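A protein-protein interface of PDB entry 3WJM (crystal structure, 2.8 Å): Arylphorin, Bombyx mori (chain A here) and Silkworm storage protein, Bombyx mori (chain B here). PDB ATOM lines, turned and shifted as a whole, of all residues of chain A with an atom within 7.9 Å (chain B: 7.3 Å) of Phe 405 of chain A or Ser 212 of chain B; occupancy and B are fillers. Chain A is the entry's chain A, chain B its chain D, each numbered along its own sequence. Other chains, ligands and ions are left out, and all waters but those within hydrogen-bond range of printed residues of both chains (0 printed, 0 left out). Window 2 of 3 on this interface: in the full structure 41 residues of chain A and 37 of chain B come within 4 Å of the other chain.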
ATOM      1  N   PRO A 402      27.778 -23.057  -4.939  1.00  0.00           N
ATOM      2  CA  PRO A 402      26.916 -22.684  -3.790  1.00  0.00           C
ATOM      3  C   PRO A 402      25.452 -22.842  -4.121  1.00  0.00           C
ATOM      4  O   PRO A 402      25.131 -22.950  -5.273  1.00  0.00           O
ATOM      5  CB  PRO A 402      27.237 -21.197  -3.567  1.00  0.00           C
ATOM      6  CG  PRO A 402      28.003 -20.750  -4.767  1.00  0.00           C
ATOM      7  CD  PRO A 402      28.710 -21.975  -5.286  1.00  0.00           C
ATOM      8  N   MET A 403      24.560 -22.850  -3.138  1.00  0.00           N
ATOM      9  CA  MET A 403      23.121 -23.030  -3.421  1.00  0.00           C
ATOM     10  C   MET A 403      22.652 -22.001  -4.435  1.00  0.00           C
ATOM     11  O   MET A 403      22.972 -20.839  -4.298  1.00  0.00           O
ATOM     12  CB  MET A 403      22.273 -22.929  -2.157  1.00  0.00           C
ATOM     13  CG  MET A 403      22.366 -24.138  -1.240  1.00  0.00           C
ATOM     14  SD  MET A 403      21.673 -25.724  -1.825  1.00  0.00           S
ATOM     15  CE  MET A 403      19.877 -25.499  -1.753  1.00  0.00           C
ATOM     16  N   PRO A 404      21.879 -22.412  -5.453  1.00  0.00           N
ATOM     17  CA  PRO A 404      21.303 -21.356  -6.319  1.00  0.00           C
ATOM     18  C   PRO A 404      20.663 -20.240  -5.504  1.00  0.00           C
ATOM     19  O   PRO A 404      20.050 -20.523  -4.485  1.00  0.00           O
ATOM     20  CB  PRO A 404      20.242 -22.096  -7.131  1.00  0.00           C
ATOM     21  CG  PRO A 404      20.707 -23.529  -7.143  1.00  0.00           C
ATOM     22  CD  PRO A 404      21.476 -23.770  -5.872  1.00  0.00           C
ATOM     23  N   PHE A 405      20.838 -18.994  -5.956  1.00  0.00           N
ATOM     24  CA  PHE A 405      20.163 -17.797  -5.411  1.00  0.00           C
ATOM     25  C   PHE A 405      18.630 -17.891  -5.499  1.00  0.00           C
ATOM     26  O   PHE A 405      17.953 -17.617  -4.530  1.00  0.00           O
ATOM     27  CB  PHE A 405      20.700 -16.552  -6.123  1.00  0.00           C
ATOM     28  CG  PHE A 405      20.054 -15.252  -5.704  1.00  0.00           C
ATOM     29  CD1 PHE A 405      18.944 -14.740  -6.398  1.00  0.00           C
ATOM     30  CD2 PHE A 405      20.591 -14.489  -4.672  1.00  0.00           C
ATOM     31  CE1 PHE A 405      18.370 -13.507  -6.045  1.00  0.00           C
ATOM     32  CE2 PHE A 405      20.014 -13.270  -4.305  1.00  0.00           C
ATOM     33  CZ  PHE A 405      18.900 -12.775  -4.992  1.00  0.00           C
ATOM     34  N   ASP A 406      18.093 -18.279  -6.658  1.00  0.00           N
ATOM     35  CA  ASP A 406      16.678 -18.624  -6.805  1.00  0.00           C
ATOM     36  C   ASP A 406      16.515 -19.533  -8.000  1.00  0.00           C
ATOM     37  O   ASP A 406      17.516 -19.853  -8.663  1.00  0.00           O
ATOM     38  CB  ASP A 406      15.790 -17.393  -6.978  1.00  0.00           C
ATOM     39  CG  ASP A 406      16.063 -16.618  -8.267  1.00  0.00           C
ATOM     40  OD1 ASP A 406      15.688 -15.436  -8.282  1.00  0.00           O
ATOM     41  OD2 ASP A 406      16.618 -17.149  -9.258  1.00  0.00           O
ATOM     42  N   LYS A 407      15.261 -19.917  -8.295  1.00  0.00           N
ATOM     43  CA  LYS A 407      14.970 -20.830  -9.403  1.00  0.00           C
ATOM     44  C   LYS A 407      15.626 -20.469 -10.784  1.00  0.00           C
ATOM     45  O   LYS A 407      15.743 -21.324 -11.652  1.00  0.00           O
ATOM     46  CB  LYS A 407      13.467 -21.012  -9.534  1.00  0.00           C
ATOM     47  CG  LYS A 407      12.775 -19.833 -10.204  1.00  0.00           C
ATOM     48  CD  LYS A 407      11.322 -19.707  -9.780  1.00  0.00           C
ATOM     49  CE  LYS A 407      10.898 -18.248  -9.767  1.00  0.00           C
ATOM     50  NZ  LYS A 407       9.686 -18.116  -8.913  1.00  0.00           N
ATOM     51  N   TYR A 408      16.068 -19.234 -10.988  1.00  0.00           N
ATOM     52  CA  TYR A 408      16.667 -18.873 -12.268  1.00  0.00           C
ATOM     53  C   TYR A 408      18.111 -18.359 -12.153  1.00  0.00           C
ATOM     54  O   TYR A 408      18.702 -17.894 -13.141  1.00  0.00           O
ATOM     55  CB  TYR A 408      15.866 -17.767 -12.949  1.00  0.00           C
ATOM     56  CG  TYR A 408      14.445 -18.063 -13.351  1.00  0.00           C
ATOM     57  CD1 TYR A 408      13.428 -17.201 -12.973  1.00  0.00           C
ATOM     58  CD2 TYR A 408      14.120 -19.153 -14.161  1.00  0.00           C
ATOM     59  CE1 TYR A 408      12.128 -17.423 -13.356  1.00  0.00           C
ATOM     60  CE2 TYR A 408      12.814 -19.388 -14.546  1.00  0.00           C
ATOM     61  CZ  TYR A 408      11.824 -18.514 -14.140  1.00  0.00           C
ATOM     62  OH  TYR A 408      10.509 -18.697 -14.511  1.00  0.00           O
ATOM     63  N   THR A 409      18.677 -18.393 -10.952  1.00  0.00           N
ATOM     64  CA  THR A 409      19.972 -17.768 -10.766  1.00  0.00           C
ATOM     65  C   THR A 409      20.808 -18.762 -10.018  1.00  0.00           C
ATOM     66  O   THR A 409      20.658 -18.933  -8.808  1.00  0.00           O
ATOM     67  CB  THR A 409      19.875 -16.407 -10.011  1.00  0.00           C
ATOM     68  OG1 THR A 409      18.718 -15.665 -10.447  1.00  0.00           O
ATOM     69  CG2 THR A 409      21.117 -15.558 -10.235  1.00  0.00           C
ATOM     70  N   PHE A 410      21.659 -19.455 -10.757  1.00  0.00           N
ATOM     71  CA  PHE A 410      22.620 -20.359 -10.150  1.00  0.00           C
ATOM     72  C   PHE A 410      24.077 -20.015 -10.477  1.00  0.00           C
ATOM     73  O   PHE A 410      24.351 -19.190 -11.336  1.00  0.00           O
ATOM     74  CB  PHE A 410      22.316 -21.789 -10.579  1.00  0.00           C
ATOM     75  CG  PHE A 410      22.470 -22.033 -12.047  1.00  0.00           C
ATOM     76  CD1 PHE A 410      21.486 -21.621 -12.950  1.00  0.00           C
ATOM     77  CD2 PHE A 410      23.578 -22.711 -12.532  1.00  0.00           C
ATOM     78  CE1 PHE A 410      21.615 -21.878 -14.313  1.00  0.00           C
ATOM     79  CE2 PHE A 410      23.707 -22.970 -13.893  1.00  0.00           C
ATOM     80  CZ  PHE A 410      22.721 -22.558 -14.789  1.00  0.00           C
ATOM     81  N   MET A 411      25.019 -20.651  -9.789  1.00  0.00           N
ATOM     82  CA  MET A 411      26.399 -20.560 -10.228  1.00  0.00           C
ATOM     83  C   MET A 411      26.813 -21.788 -11.050  1.00  0.00           C
ATOM     84  O   MET A 411      26.917 -22.930 -10.527  1.00  0.00           O
ATOM     85  CB  MET A 411      27.360 -20.310  -9.085  1.00  0.00           C
ATOM     86  CG  MET A 411      28.592 -19.630  -9.617  1.00  0.00           C
ATOM     87  SD  MET A 411      30.012 -19.985  -8.607  1.00  0.00           S
ATOM     88  CE  MET A 411      30.944 -18.497  -8.979  1.00  0.00           C
ATOM     89  N   TYR B 209      25.322  -4.365  -5.302  1.00  0.00           N
ATOM     90  CA  TYR B 209      26.282  -5.201  -4.607  1.00  0.00           C
ATOM     91  C   TYR B 209      25.969  -6.684  -4.833  1.00  0.00           C
ATOM     92  O   TYR B 209      24.844  -7.057  -5.155  1.00  0.00           O
ATOM     93  CB  TYR B 209      26.240  -4.848  -3.144  1.00  0.00           C
ATOM     94  CG  TYR B 209      26.709  -3.445  -2.903  1.00  0.00           C
ATOM     95  CD1 TYR B 209      28.070  -3.146  -2.914  1.00  0.00           C
ATOM     96  CD2 TYR B 209      25.803  -2.413  -2.648  1.00  0.00           C
ATOM     97  CE1 TYR B 209      28.537  -1.886  -2.665  1.00  0.00           C
ATOM     98  CE2 TYR B 209      26.264  -1.117  -2.414  1.00  0.00           C
ATOM     99  CZ  TYR B 209      27.648  -0.868  -2.440  1.00  0.00           C
ATOM    100  OH  TYR B 209      28.152   0.410  -2.263  1.00  0.00           O
ATOM    101  N   SER B 210      26.963  -7.539  -4.690  1.00  0.00           N
ATOM    102  CA  SER B 210      26.786  -8.936  -4.993  1.00  0.00           C
ATOM    103  C   SER B 210      25.883  -9.695  -4.035  1.00  0.00           C
ATOM    104  O   SER B 210      25.661  -9.281  -2.899  1.00  0.00           O
ATOM    105  CB  SER B 210      28.116  -9.643  -5.136  1.00  0.00           C
ATOM    106  OG  SER B 210      29.188  -8.856  -4.707  1.00  0.00           O
ATOM    107  N   ASN B 211      25.318 -10.788  -4.532  1.00  0.00           N
ATOM    108  CA  ASN B 211      24.390 -11.533  -3.745  1.00  0.00           C
ATOM    109  C   ASN B 211      24.950 -12.851  -3.173  1.00  0.00           C
ATOM    110  O   ASN B 211      26.176 -13.067  -3.120  1.00  0.00           O
ATOM    111  CB  ASN B 211      23.076 -11.737  -4.514  1.00  0.00           C
ATOM    112  CG  ASN B 211      23.250 -12.453  -5.876  1.00  0.00           C
ATOM    113  OD1 ASN B 211      24.267 -13.078  -6.174  1.00  0.00           O
ATOM    114  ND2 ASN B 211      22.197 -12.364  -6.704  1.00  0.00           N
ATOM    115  N   SER B 212      24.036 -13.717  -2.741  1.00  0.00           N
ATOM    116  CA  SER B 212      24.375 -14.952  -2.092  1.00  0.00           C
ATOM    117  C   SER B 212      25.316 -15.841  -2.935  1.00  0.00           C
ATOM    118  O   SER B 212      26.023 -16.695  -2.390  1.00  0.00           O
ATOM    119  CB  SER B 212      23.095 -15.662  -1.642  1.00  0.00           C
ATOM    120  OG  SER B 212      22.629 -16.618  -2.577  1.00  0.00           O
ATOM    121  N   LEU B 213      25.371 -15.622  -4.249  1.00  0.00           N
ATOM    122  CA  LEU B 213      26.340 -16.353  -5.085  1.00  0.00           C
ATOM    123  C   LEU B 213      27.819 -15.997  -4.890  1.00  0.00           C
ATOM    124  O   LEU B 213      28.650 -16.831  -5.186  1.00  0.00           O
ATOM    125  CB  LEU B 213      25.988 -16.278  -6.574  1.00  0.00           C
ATOM    126  CG  LEU B 213      24.759 -17.156  -6.886  1.00  0.00           C
ATOM    127  CD1 LEU B 213      24.480 -17.203  -8.392  1.00  0.00           C
ATOM    128  CD2 LEU B 213      24.844 -18.551  -6.244  1.00  0.00           C
ATOM    129  N   THR B 214      28.176 -14.784  -4.440  1.00  0.00           N
ATOM    130  CA  THR B 214      29.598 -14.532  -4.156  1.00  0.00           C
ATOM    131  C   THR B 214      29.952 -14.570  -2.657  1.00  0.00           C
ATOM    132  O   THR B 214      31.065 -14.893  -2.279  1.00  0.00           O
ATOM    133  CB  THR B 214      30.174 -13.276  -4.860  1.00  0.00           C
ATOM    134  OG1 THR B 214      29.667 -12.089  -4.279  1.00  0.00           O
ATOM    135  CG2 THR B 214      29.847 -13.281  -6.344  1.00  0.00           C
ATOM    136  N   TYR B 215      28.972 -14.256  -1.826  1.00  0.00           N
ATOM    137  CA  TYR B 215      29.080 -14.336  -0.374  1.00  0.00           C
ATOM    138  C   TYR B 215      28.085 -15.398   0.079  1.00  0.00           C
ATOM    139  O   TYR B 215      26.976 -15.054   0.517  1.00  0.00           O
ATOM    140  CB  TYR B 215      28.690 -12.989   0.270  1.00  0.00           C
ATOM    141  CG  TYR B 215      29.667 -11.883   0.054  1.00  0.00           C
ATOM    142  CD1 TYR B 215      29.365 -10.815  -0.764  1.00  0.00           C
ATOM    143  CD2 TYR B 215      30.903 -11.919   0.660  1.00  0.00           C
ATOM    144  CE1 TYR B 215      30.283  -9.797  -0.972  1.00  0.00           C
ATOM    145  CE2 TYR B 215      31.829 -10.911   0.469  1.00  0.00           C
ATOM    146  CZ  TYR B 215      31.522  -9.864  -0.348  1.00  0.00           C
ATOM    147  OH  TYR B 215      32.468  -8.895  -0.539  1.00  0.00           O
ATOM    148  N   PRO B 216      28.455 -16.687  -0.054  1.00  0.00           N
ATOM    149  CA  PRO B 216      27.466 -17.749   0.179  1.00  0.00           C
ATOM    150  C   PRO B 216      27.126 -17.973   1.658  1.00  0.00           C
ATOM    151  O   PRO B 216      27.091 -19.116   2.105  1.00  0.00           O
ATOM    152  CB  PRO B 216      28.111 -18.990  -0.447  1.00  0.00           C
ATOM    153  CG  PRO B 216      29.584 -18.695  -0.470  1.00  0.00           C
ATOM    154  CD  PRO B 216      29.804 -17.219  -0.310  1.00  0.00           C
ATOM    155  N   ASN B 217      26.863 -16.886   2.387  1.00  0.00           N
ATOM    156  CA  ASN B 217      26.524 -16.951   3.796  1.00  0.00           C
ATOM    157  C   ASN B 217      26.078 -15.593   4.301  1.00  0.00           C
ATOM    158  O   ASN B 217      25.900 -14.688   3.526  1.00  0.00           O
ATOM    159  CB  ASN B 217      27.739 -17.411   4.591  1.00  0.00           C
ATOM    160  CG  ASN B 217      28.989 -16.671   4.183  1.00  0.00           C
ATOM    161  OD1 ASN B 217      29.908 -17.263   3.665  1.00  0.00           O
ATOM    162  ND2 ASN B 217      28.985 -15.357   4.333  1.00  0.00           N
ATOM    163  N   ASP B 220      26.992 -11.794   3.431  1.00  0.00           N
ATOM    164  CA  ASP B 220      26.344 -11.027   2.400  1.00  0.00           C
ATOM    165  C   ASP B 220      25.496  -9.883   2.959  1.00  0.00           C
ATOM    166  O   ASP B 220      25.258  -8.888   2.284  1.00  0.00           O
ATOM    167  CB  ASP B 220      25.491 -11.921   1.512  1.00  0.00           C
ATOM    168  CG  ASP B 220      25.144 -11.262   0.148  1.00  0.00           C
ATOM    169  OD1 ASP B 220      25.887 -10.369  -0.318  1.00  0.00           O
ATOM    170  OD2 ASP B 220      24.132 -11.674  -0.460  1.00  0.00           O
ATOM    171  N   LEU B 299      33.359 -16.060  -3.075  1.00  0.00           N
ATOM    172  CA  LEU B 299      33.702 -16.280  -4.480  1.00  0.00           C
ATOM    173  C   LEU B 299      33.820 -14.925  -5.203  1.00  0.00           C
ATOM    174  O   LEU B 299      32.811 -14.314  -5.525  1.00  0.00           O
ATOM    175  CB  LEU B 299      32.730 -17.216  -5.172  1.00  0.00           C
ATOM    176  CG  LEU B 299      31.766 -18.162  -4.461  1.00  0.00           C
ATOM    177  CD1 LEU B 299      31.258 -19.124  -5.513  1.00  0.00           C
ATOM    178  CD2 LEU B 299      32.345 -18.931  -3.291  1.00  0.00           C
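The backbone NH (N) of Leu 213 of chain B sits close to the side-chain amide oxygen (OD1) of Asn 211 of chain B (3.4 Å). The backbone NH (N) of Ser 212 of chain B sits at hydrogen-bond distance from the side-chain carboxylate (OD2) of Asp 220 of chain B (3.1 Å). The backbone NH (N) of Leu 299 of chain B lies within hydrogen-bond range of the backbone carbonyl oxygen (O) of Thr 214 of chain B, 2.7 Å away.
Hydrophobic or aromatic side chains of chain A that line the printed part of chain B: Pro 402, Phe 405 and Met 411. Hydrophobic or aromatic side chains of chain B within 4 Å of the printed part of chain A: Leu 213, Pro 216 and Leu 299. Along chain B the printed residues that touch a printed residue of chain A span positions 211 to 299. Among the printed residues, 9 pairs touch across the chains.
Ser 212 of chain B touches just one residue of chain A: Phe 405 (3.6 Å). Printed residues of chain A within 4 Å of Asn 211 of chain B: Phe 405 (3.4 Å). Printed residues of chain A within 4 Å of Leu 213 of chain B: Pro 402 (3.99 Å), Met 403 (3.5 Å), Phe 410 (3.5 Å) and Met 411 (3.8 Å). Printed residues of chain B within 4 Å of Met 411 of chain A: Leu 213 and Leu 299. Printed residues of chain B within 4 Å of Pro 402 of chain A: Leu 213, Pro 216 and Leu 299. Of the printed residues of chain B, Met 403 of chain A touches Leu 213. Thr 214 of chain B touches none of the printed residues of chain A. Ser 210 of chain B touches none of the printed residues of chain A. The nearest residue of chain A that does not touch Ser 212 of chain B is Met 403 of chain A (4.6 Å).
Among the printed residues, merely in contact across the chains: Phe 405 of chain A with Asn 211 of chain B, Met 411 of chain A with Leu 299 of chain B, Phe 410 of chain A with Leu 213 of chain B, Met 403 of chain A with Leu 213 of chain B, Phe 405 of chain A with Ser 212 of chain B, Pro 402 of chain A with Leu 299 of chain B, Met 411 of chain A with Leu 213 of chain B, Pro 402 of chain A with Pro 216 of chain B and Pro 402 of chain A with Leu 213 of chain B.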
